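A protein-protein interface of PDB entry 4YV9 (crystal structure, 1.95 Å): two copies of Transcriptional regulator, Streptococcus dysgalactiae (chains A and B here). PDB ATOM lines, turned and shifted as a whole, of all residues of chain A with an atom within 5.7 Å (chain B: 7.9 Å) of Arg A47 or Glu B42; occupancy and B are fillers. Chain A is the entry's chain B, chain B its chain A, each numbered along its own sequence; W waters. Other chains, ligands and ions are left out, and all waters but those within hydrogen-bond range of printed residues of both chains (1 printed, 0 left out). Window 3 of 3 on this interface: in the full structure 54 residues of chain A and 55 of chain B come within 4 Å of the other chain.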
ATOM      1  N   GLU A  26      12.072   0.566  14.278  1.00  0.00           N
ATOM      2  CA  GLU A  26      12.653   0.831  12.967  1.00  0.00           C
ATOM      3  C   GLU A  26      14.116   1.281  13.014  1.00  0.00           C
ATOM      4  O   GLU A  26      14.801   1.258  11.997  1.00  0.00           O
ATOM      5  CB  GLU A  26      11.827   1.894  12.234  1.00  0.00           C
ATOM      6  CG  GLU A  26      11.671   3.191  13.013  1.00  0.00           C
ATOM      7  CD  GLU A  26      10.900   4.255  12.247  1.00  0.00           C
ATOM      8  OE1 GLU A  26      10.867   4.196  10.994  1.00  0.00           O
ATOM      9  OE2 GLU A  26      10.323   5.150  12.904  1.00  0.00           O
ATOM     10  N   HIS A  27      14.589   1.704  14.180  1.00  0.00           N
ATOM     11  CA  HIS A  27      15.949   2.229  14.297  1.00  0.00           C
ATOM     12  C   HIS A  27      16.957   1.141  14.680  1.00  0.00           C
ATOM     13  O   HIS A  27      18.096   1.162  14.229  1.00  0.00           O
ATOM     14  CB  HIS A  27      15.995   3.375  15.323  1.00  0.00           C
ATOM     15  CG  HIS A  27      14.937   4.416  15.113  1.00  0.00           C
ATOM     16  ND1 HIS A  27      14.980   5.321  14.074  1.00  0.00           N
ATOM     17  CD2 HIS A  27      13.798   4.684  15.799  1.00  0.00           C
ATOM     18  CE1 HIS A  27      13.916   6.102  14.129  1.00  0.00           C
ATOM     19  NE2 HIS A  27      13.184   5.738  15.167  1.00  0.00           N
ATOM     20  N   LEU A  28      16.534   0.203  15.518  1.00  0.00           N
ATOM     21  CA  LEU A  28      17.402  -0.889  15.951  1.00  0.00           C
ATOM     22  C   LEU A  28      16.624  -2.187  16.056  1.00  0.00           C
ATOM     23  O   LEU A  28      15.595  -2.227  16.704  1.00  0.00           O
ATOM     24  CB  LEU A  28      18.048  -0.582  17.310  1.00  0.00           C
ATOM     25  CG  LEU A  28      19.347   0.214  17.379  1.00  0.00           C
ATOM     26  CD1 LEU A  28      19.843   0.296  18.838  1.00  0.00           C
ATOM     27  CD2 LEU A  28      20.427  -0.365  16.478  1.00  0.00           C
ATOM     28  N   ILE A  43      26.772   0.511  18.490  1.00  0.00           N
ATOM     29  CA  ILE A  43      25.644   1.286  17.983  1.00  0.00           C
ATOM     30  C   ILE A  43      25.911   2.771  18.180  1.00  0.00           C
ATOM     31  O   ILE A  43      26.782   3.160  18.972  1.00  0.00           O
ATOM     32  CB  ILE A  43      24.323   0.916  18.680  1.00  0.00           C
ATOM     33  CG1 ILE A  43      24.436   1.148  20.195  1.00  0.00           C
ATOM     34  CG2 ILE A  43      23.933  -0.523  18.366  1.00  0.00           C
ATOM     35  CD1 ILE A  43      23.097   1.039  20.919  1.00  0.00           C
ATOM     36  N   SER A  44      25.173   3.609  17.462  1.00  0.00           N
ATOM     37  CA  SER A  44      25.402   5.040  17.559  1.00  0.00           C
ATOM     38  C   SER A  44      24.895   5.551  18.894  1.00  0.00           C
ATOM     39  O   SER A  44      24.033   4.930  19.529  1.00  0.00           O
ATOM     40  CB  SER A  44      24.723   5.786  16.416  1.00  0.00           C
ATOM     41  OG  SER A  44      23.321   5.826  16.593  1.00  0.00           O
ATOM     42  N   CYS A  45      25.432   6.682  19.330  1.00  0.00           N
ATOM     43  CA  CYS A  45      24.992   7.264  20.587  1.00  0.00           C
ATOM     44  C   CYS A  45      23.502   7.577  20.499  1.00  0.00           C
ATOM     45  O   CYS A  45      22.741   7.298  21.427  1.00  0.00           O
ATOM     46  CB  CYS A  45      25.786   8.525  20.917  1.00  0.00           C
ATOM     47  SG  CYS A  45      25.555   9.046  22.642  1.00  0.00           S
ATOM     48  N   SER A  46      23.100   8.147  19.369  1.00  0.00           N
ATOM     49  CA  SER A  46      21.704   8.496  19.126  1.00  0.00           C
ATOM     50  C   SER A  46      20.789   7.284  19.293  1.00  0.00           C
ATOM     51  O   SER A  46      19.729   7.371  19.890  1.00  0.00           O
ATOM     52  CB  SER A  46      21.547   9.092  17.724  1.00  0.00           C
ATOM     53  OG  SER A  46      20.466  10.010  17.691  1.00  0.00           O
ATOM     54  N   ARG A  47      21.211   6.138  18.785  1.00  0.00           N
ATOM     55  CA  ARG A  47      20.381   4.950  18.906  1.00  0.00           C
ATOM     56  C   ARG A  47      20.389   4.430  20.343  1.00  0.00           C
ATOM     57  O   ARG A  47      19.370   3.928  20.836  1.00  0.00           O
ATOM     58  CB  ARG A  47      20.836   3.891  17.898  1.00  0.00           C
ATOM     59  CG  ARG A  47      20.376   4.259  16.498  1.00  0.00           C
ATOM     60  CD  ARG A  47      21.071   3.484  15.389  1.00  0.00           C
ATOM     61  NE  ARG A  47      20.131   3.170  14.316  1.00  0.00           N
ATOM     62  CZ  ARG A  47      19.963   3.896  13.216  1.00  0.00           C
ATOM     63  NH1 ARG A  47      20.687   4.986  13.014  1.00  0.00           N
ATOM     64  NH2 ARG A  47      19.074   3.520  12.308  1.00  0.00           N
ATOM     65  N   LEU A  48      21.519   4.586  21.032  1.00  0.00           N
ATOM     66  CA  LEU A  48      21.575   4.239  22.446  1.00  0.00           C
ATOM     67  C   LEU A  48      20.630   5.123  23.254  1.00  0.00           C
ATOM     68  O   LEU A  48      19.901   4.633  24.123  1.00  0.00           O
ATOM     69  CB  LEU A  48      23.000   4.370  22.994  1.00  0.00           C
ATOM     70  CG  LEU A  48      23.149   4.093  24.495  1.00  0.00           C
ATOM     71  CD1 LEU A  48      22.576   2.736  24.872  1.00  0.00           C
ATOM     72  CD2 LEU A  48      24.615   4.172  24.889  1.00  0.00           C
ATOM     73  N   LEU A  49      20.635   6.420  22.962  1.00  0.00           N
ATOM     74  CA  LEU A  49      19.745   7.354  23.669  1.00  0.00           C
ATOM     75  C   LEU A  49      18.276   7.004  23.514  1.00  0.00           C
ATOM     76  O   LEU A  49      17.499   7.180  24.449  1.00  0.00           O
ATOM     77  CB  LEU A  49      19.966   8.785  23.194  1.00  0.00           C
ATOM     78  CG  LEU A  49      20.853   9.646  24.100  1.00  0.00           C
ATOM     79  CD1 LEU A  49      22.223   9.034  24.270  1.00  0.00           C
ATOM     80  CD2 LEU A  49      20.975  11.041  23.540  1.00  0.00           C
ATOM     81  N   ASN A  50      17.907   6.537  22.324  1.00  0.00           N
ATOM     82  CA  ASN A  50      16.550   6.061  22.041  1.00  0.00           C
ATOM     83  C   ASN A  50      16.179   4.880  22.940  1.00  0.00           C
ATOM     84  O   ASN A  50      15.084   4.835  23.501  1.00  0.00           O
ATOM     85  CB  ASN A  50      16.443   5.666  20.556  1.00  0.00           C
ATOM     86  CG  ASN A  50      15.014   5.288  20.123  1.00  0.00           C
ATOM     87  OD1 ASN A  50      14.041   5.925  20.509  1.00  0.00           O
ATOM     88  ND2 ASN A  50      14.904   4.248  19.298  1.00  0.00           N
ATOM     89  N   LEU A  51      17.098   3.923  23.065  1.00  0.00           N
ATOM     90  CA  LEU A  51      16.911   2.772  23.953  1.00  0.00           C
ATOM     91  C   LEU A  51      16.740   3.203  25.396  1.00  0.00           C
ATOM     92  O   LEU A  51      15.842   2.736  26.104  1.00  0.00           O
ATOM     93  CB  LEU A  51      18.102   1.812  23.864  1.00  0.00           C
ATOM     94  CG  LEU A  51      18.387   1.123  22.545  1.00  0.00           C
ATOM     95  CD1 LEU A  51      19.721   0.346  22.618  1.00  0.00           C
ATOM     96  CD2 LEU A  51      17.235   0.192  22.201  1.00  0.00           C
ATOM     97  N   LEU A  52      17.636   4.074  25.841  1.00  0.00           N
ATOM     98  CA  LEU A  52      17.597   4.596  27.197  1.00  0.00           C
ATOM     99  C   LEU A  52      16.290   5.327  27.509  1.00  0.00           C
ATOM    100  O   LEU A  52      15.713   5.172  28.587  1.00  0.00           O
ATOM    101  CB  LEU A  52      18.771   5.542  27.412  1.00  0.00           C
ATOM    102  CG  LEU A  52      20.127   4.835  27.428  1.00  0.00           C
ATOM    103  CD1 LEU A  52      21.237   5.827  27.761  1.00  0.00           C
ATOM    104  CD2 LEU A  52      20.079   3.704  28.443  1.00  0.00           C
ATOM    105  N   LEU B   5      21.942  15.395  18.132  1.00  0.00           N
ATOM    106  CA  LEU B   5      23.082  15.515  19.040  1.00  0.00           C
ATOM    107  C   LEU B   5      24.236  16.263  18.390  1.00  0.00           C
ATOM    108  O   LEU B   5      24.980  16.973  19.066  1.00  0.00           O
ATOM    109  CB  LEU B   5      23.565  14.136  19.499  1.00  0.00           C
ATOM    110  CG  LEU B   5      22.664  13.313  20.418  1.00  0.00           C
ATOM    111  CD1 LEU B   5      23.216  11.904  20.566  1.00  0.00           C
ATOM    112  CD2 LEU B   5      22.552  13.992  21.773  1.00  0.00           C
ATOM    113  N   LEU B  28      38.739  11.019  16.620  1.00  0.00           N
ATOM    114  CA  LEU B  28      38.123  11.647  15.456  1.00  0.00           C
ATOM    115  C   LEU B  28      39.087  12.606  14.761  1.00  0.00           C
ATOM    116  O   LEU B  28      40.112  12.998  15.321  1.00  0.00           O
ATOM    117  CB  LEU B  28      36.844  12.397  15.852  1.00  0.00           C
ATOM    118  CG  LEU B  28      35.506  11.645  15.853  1.00  0.00           C
ATOM    119  CD1 LEU B  28      35.187  11.145  17.245  1.00  0.00           C
ATOM    120  CD2 LEU B  28      34.374  12.521  15.342  1.00  0.00           C
ATOM    121  N   GLN B  32      35.541  14.343  10.624  1.00  0.00           N
ATOM    122  CA  GLN B  32      34.464  13.618  11.290  1.00  0.00           C
ATOM    123  C   GLN B  32      33.827  14.413  12.414  1.00  0.00           C
ATOM    124  O   GLN B  32      32.614  14.341  12.620  1.00  0.00           O
ATOM    125  CB  GLN B  32      34.986  12.304  11.838  1.00  0.00           C
ATOM    126  CG  GLN B  32      35.408  11.329  10.780  1.00  0.00           C
ATOM    127  CD  GLN B  32      36.003  10.107  11.399  1.00  0.00           C
ATOM    128  OE1 GLN B  32      36.966  10.213  12.151  1.00  0.00           O
ATOM    129  NE2 GLN B  32      35.455   8.938  11.089  1.00  0.00           N
ATOM    130  N   ARG B  35      31.888  16.504  10.817  1.00  0.00           N
ATOM    131  CA  ARG B  35      30.901  15.731  10.088  1.00  0.00           C
ATOM    132  C   ARG B  35      29.783  15.269  11.041  1.00  0.00           C
ATOM    133  O   ARG B  35      28.615  15.180  10.652  1.00  0.00           O
ATOM    134  CB  ARG B  35      31.582  14.559   9.361  1.00  0.00           C
ATOM    135  CG  ARG B  35      31.359  14.628   7.885  1.00  0.00           C
ATOM    136  CD  ARG B  35      32.140  13.726   6.963  1.00  0.00           C
ATOM    137  NE  ARG B  35      33.574  13.587   7.165  1.00  0.00           N
ATOM    138  CZ  ARG B  35      34.187  12.418   7.083  1.00  0.00           C
ATOM    139  NH1 ARG B  35      33.471  11.345   6.815  1.00  0.00           N
ATOM    140  NH2 ARG B  35      35.493  12.321   7.254  1.00  0.00           N
ATOM    141  N   PHE B  36      30.131  15.045  12.307  1.00  0.00           N
ATOM    142  CA  PHE B  36      29.126  14.700  13.310  1.00  0.00           C
ATOM    143  C   PHE B  36      28.285  15.910  13.660  1.00  0.00           C
ATOM    144  O   PHE B  36      27.077  15.790  13.844  1.00  0.00           O
ATOM    145  CB  PHE B  36      29.769  14.138  14.583  1.00  0.00           C
ATOM    146  CG  PHE B  36      28.795  13.929  15.708  1.00  0.00           C
ATOM    147  CD1 PHE B  36      27.837  12.927  15.644  1.00  0.00           C
ATOM    148  CD2 PHE B  36      28.823  14.750  16.824  1.00  0.00           C
ATOM    149  CE1 PHE B  36      26.933  12.739  16.680  1.00  0.00           C
ATOM    150  CE2 PHE B  36      27.923  14.567  17.865  1.00  0.00           C
ATOM    151  CZ  PHE B  36      26.978  13.560  17.790  1.00  0.00           C
ATOM    152  N   GLY B  39      25.263  16.834  11.735  1.00  0.00           N
ATOM    153  CA  GLY B  39      24.244  15.802  11.810  1.00  0.00           C
ATOM    154  C   GLY B  39      24.233  14.845  10.637  1.00  0.00           C
ATOM    155  O   GLY B  39      23.191  14.336  10.239  1.00  0.00           O
ATOM    156  N   GLU B  40      25.401  14.604  10.074  1.00  0.00           N
ATOM    157  CA  GLU B  40      25.529  13.678   8.964  1.00  0.00           C
ATOM    158  C   GLU B  40      26.030  12.293   9.392  1.00  0.00           C
ATOM    159  O   GLU B  40      25.551  11.267   8.901  1.00  0.00           O
ATOM    160  CB  GLU B  40      26.431  14.308   7.912  1.00  0.00           C
ATOM    161  CG  GLU B  40      27.639  13.500   7.523  1.00  0.00           C
ATOM    162  CD  GLU B  40      28.438  14.139   6.417  1.00  0.00           C
ATOM    163  OE1 GLU B  40      28.790  15.313   6.576  1.00  0.00           O
ATOM    164  OE2 GLU B  40      28.816  13.416   5.494  1.00  0.00           O
ATOM    165  N   SER B  41      26.973  12.258  10.321  1.00  0.00           N
ATOM    166  CA  SER B  41      27.522  10.996  10.757  1.00  0.00           C
ATOM    167  C   SER B  41      27.082  10.715  12.182  1.00  0.00           C
ATOM    168  O   SER B  41      26.945  11.623  12.998  1.00  0.00           O
ATOM    169  CB  SER B  41      29.045  11.015  10.651  1.00  0.00           C
ATOM    170  OG  SER B  41      29.622   9.882  11.279  1.00  0.00           O
ATOM    171  N   GLU B  42      26.831   9.448  12.467  1.00  0.00           N
ATOM    172  CA  GLU B  42      26.552   9.039  13.825  1.00  0.00           C
ATOM    173  C   GLU B  42      27.869   8.682  14.486  1.00  0.00           C
ATOM    174  O   GLU B  42      28.715   8.025  13.885  1.00  0.00           O
ATOM    175  CB  GLU B  42      25.580   7.860  13.848  1.00  0.00           C
ATOM    176  CG  GLU B  42      24.175   8.203  13.371  1.00  0.00           C
ATOM    177  CD  GLU B  42      23.231   7.014  13.418  1.00  0.00           C
ATOM    178  OE1 GLU B  42      23.505   6.000  12.738  1.00  0.00           O
ATOM    179  OE2 GLU B  42      22.215   7.096  14.141  1.00  0.00           O
ATOM    180  N   ILE B  43      28.065   9.138  15.712  1.00  0.00           N
ATOM    181  CA  ILE B  43      29.242   8.723  16.446  1.00  0.00           C
ATOM    182  C   ILE B  43      28.814   7.946  17.670  1.00  0.00           C
ATOM    183  O   ILE B  43      27.689   8.085  18.137  1.00  0.00           O
ATOM    184  CB  ILE B  43      30.119   9.909  16.855  1.00  0.00           C
ATOM    185  CG1 ILE B  43      29.428  10.753  17.927  1.00  0.00           C
ATOM    186  CG2 ILE B  43      30.481  10.742  15.636  1.00  0.00           C
ATOM    187  CD1 ILE B  43      30.291  11.885  18.440  1.00  0.00           C
ATOM    188  N   SER B  44      29.710   7.106  18.168  1.00  0.00           N
ATOM    189  CA  SER B  44      29.450   6.337  19.372  1.00  0.00           C
ATOM    190  C   SER B  44      29.344   7.259  20.591  1.00  0.00           C
ATOM    191  O   SER B  44      29.825   8.398  20.568  1.00  0.00           O
ATOM    192  CB  SER B  44      30.556   5.302  19.590  1.00  0.00           C
ATOM    193  OG  SER B  44      31.742   5.933  20.054  1.00  0.00           O
ATOM    194  N   CYS B  45      28.714   6.778  21.657  1.00  0.00           N
ATOM    195  CA  CYS B  45      28.685   7.563  22.894  1.00  0.00           C
ATOM    196  C   CYS B  45      30.078   7.649  23.466  1.00  0.00           C
ATOM    197  O   CYS B  45      30.427   8.630  24.116  1.00  0.00           O
ATOM    198  CB  CYS B  45      27.737   6.955  23.919  1.00  0.00           C
ATOM    199  SG  CYS B  45      26.004   7.283  23.568  1.00  0.00           S
ATOM    200  N   ARG B  47      32.877   8.091  21.805  1.00  0.00           N
ATOM    201  CA  ARG B  47      33.564   9.202  21.158  1.00  0.00           C
ATOM    202  C   ARG B  47      32.922  10.543  21.524  1.00  0.00           C
ATOM    203  O   ARG B  47      33.613  11.548  21.674  1.00  0.00           O
ATOM    204  CB  ARG B  47      33.591   8.999  19.641  1.00  0.00           C
ATOM    205  CG  ARG B  47      34.249   7.682  19.229  1.00  0.00           C
ATOM    206  CD  ARG B  47      34.742   7.706  17.781  1.00  0.00           C
ATOM    207  NE  ARG B  47      35.170   6.401  17.274  1.00  0.00           N
ATOM    208  CZ  ARG B  47      36.186   5.688  17.754  1.00  0.00           C
ATOM    209  NH1 ARG B  47      36.909   6.137  18.772  1.00  0.00           N
ATOM    210  NH2 ARG B  47      36.483   4.517  17.210  1.00  0.00           N
HETATM  211  O   HOH W   1      24.906   9.438  17.122  1.00  0.00           O
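The guanidinium group (NH1) of Arg A47 is in salt-bridge range of the side-chain carboxylate (OE2) of Glu B42, 2.8 Å away.
The side-chain sulfur (SG) of Cys B45 is disulfide-bonded to the side-chain sulfur (SG) of Cys A45, 2.0 Å away.
The backbone carbonyl oxygen (O) of Ile B43 is in hydrogen-bond range of the backbone NH (N) of Cys A45 (2.9 Å).
The side-chain hydroxyl (OG) of Ser A44 lies within hydrogen-bond range of the side-chain carboxylate (OE2) of Glu B42, 3.0 Å away.
The backbone NH (N) of Arg A47 is in hydrogen-bond range of the side-chain hydroxyl (OG) of Ser A44, 3.1 Å away.
OG of Ser B44 sits at hydrogen-bond distance from N of Arg B47.
The backbone carbonyl oxygen of His A27 is in hydrogen-bond range of the guanidinium group of Arg A47, 2.9 Å away.
Ile B43 touches Ser A44.
C of Ser B44 touches CB of Cys A45, 3.8 Å away.
N of Ser A46 touches CD1 of Leu B5 (3.9 Å).
Leu A48 touches Cys B45.
CD2 of Leu B5 touches CD2 of Leu A49 (3.8 Å).
Of chain B, only Glu B42 comes within 4 Å of Arg A47.
Printed residues of chain A within 4 Å of Leu B5: Ser A46 and Leu A49.
Printed residues of chain B within 4 Å of Cys A45: Ile B43, Ser B44 and Cys B45.
Of the printed residues of chain B, Ser A44 touches Glu B42 (3.0 Å) and Ile B43 (3.8 Å).
Of the printed residues of chain B, Ser A46 touches Leu B5.
Of the printed residues of chain A, Ser B44 touches Cys A45 (3.8 Å).
Leu A28 touches none of the printed residues of chain B.
Arg B47 touches none of the printed residues of chain A.
The nearest residue of chain A that does not touch Glu B42 is Ser A46 (4.2 Å).
Of the 13 printed residues of chain A, 6 touch a printed residue of chain B.
Of the 13 printed residues of chain B, 5 touch a printed residue of chain A.
Hydrophobic or aromatic side chains of chain B that line the printed part of chain A: Leu B5.
Among the printed residues, Asp or Glu carboxylates within 4 Å of a Lys or Arg side-chain nitrogen of the other chain: Arg A47 with Glu B42 (2.8 Å).
Ser A44 touches Ile B43, but with the chains exchanged Ile A43 does not touch Ser B44 (4.2 Å).
Cys A45 touches Ile B43, but with the chains exchanged Ile A43 does not touch Cys B45 (4.9 Å).
Cys A45 touches Ser B44, but with the chains exchanged Ser A44 does not touch Cys B45 (4.9 Å).
Cys B45 touches its own counterpart, Cys A45.
Positions printed for both chains: 28, 43, 44, 45 and 47.
Of the 9 pairs that touch across the chains among the printed residues, 1 has its exchanged pair printed and touching as well.
Water W1 bridges N of Ser A46 (3.2 Å) and O of Ile B43 (3.3 Å).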
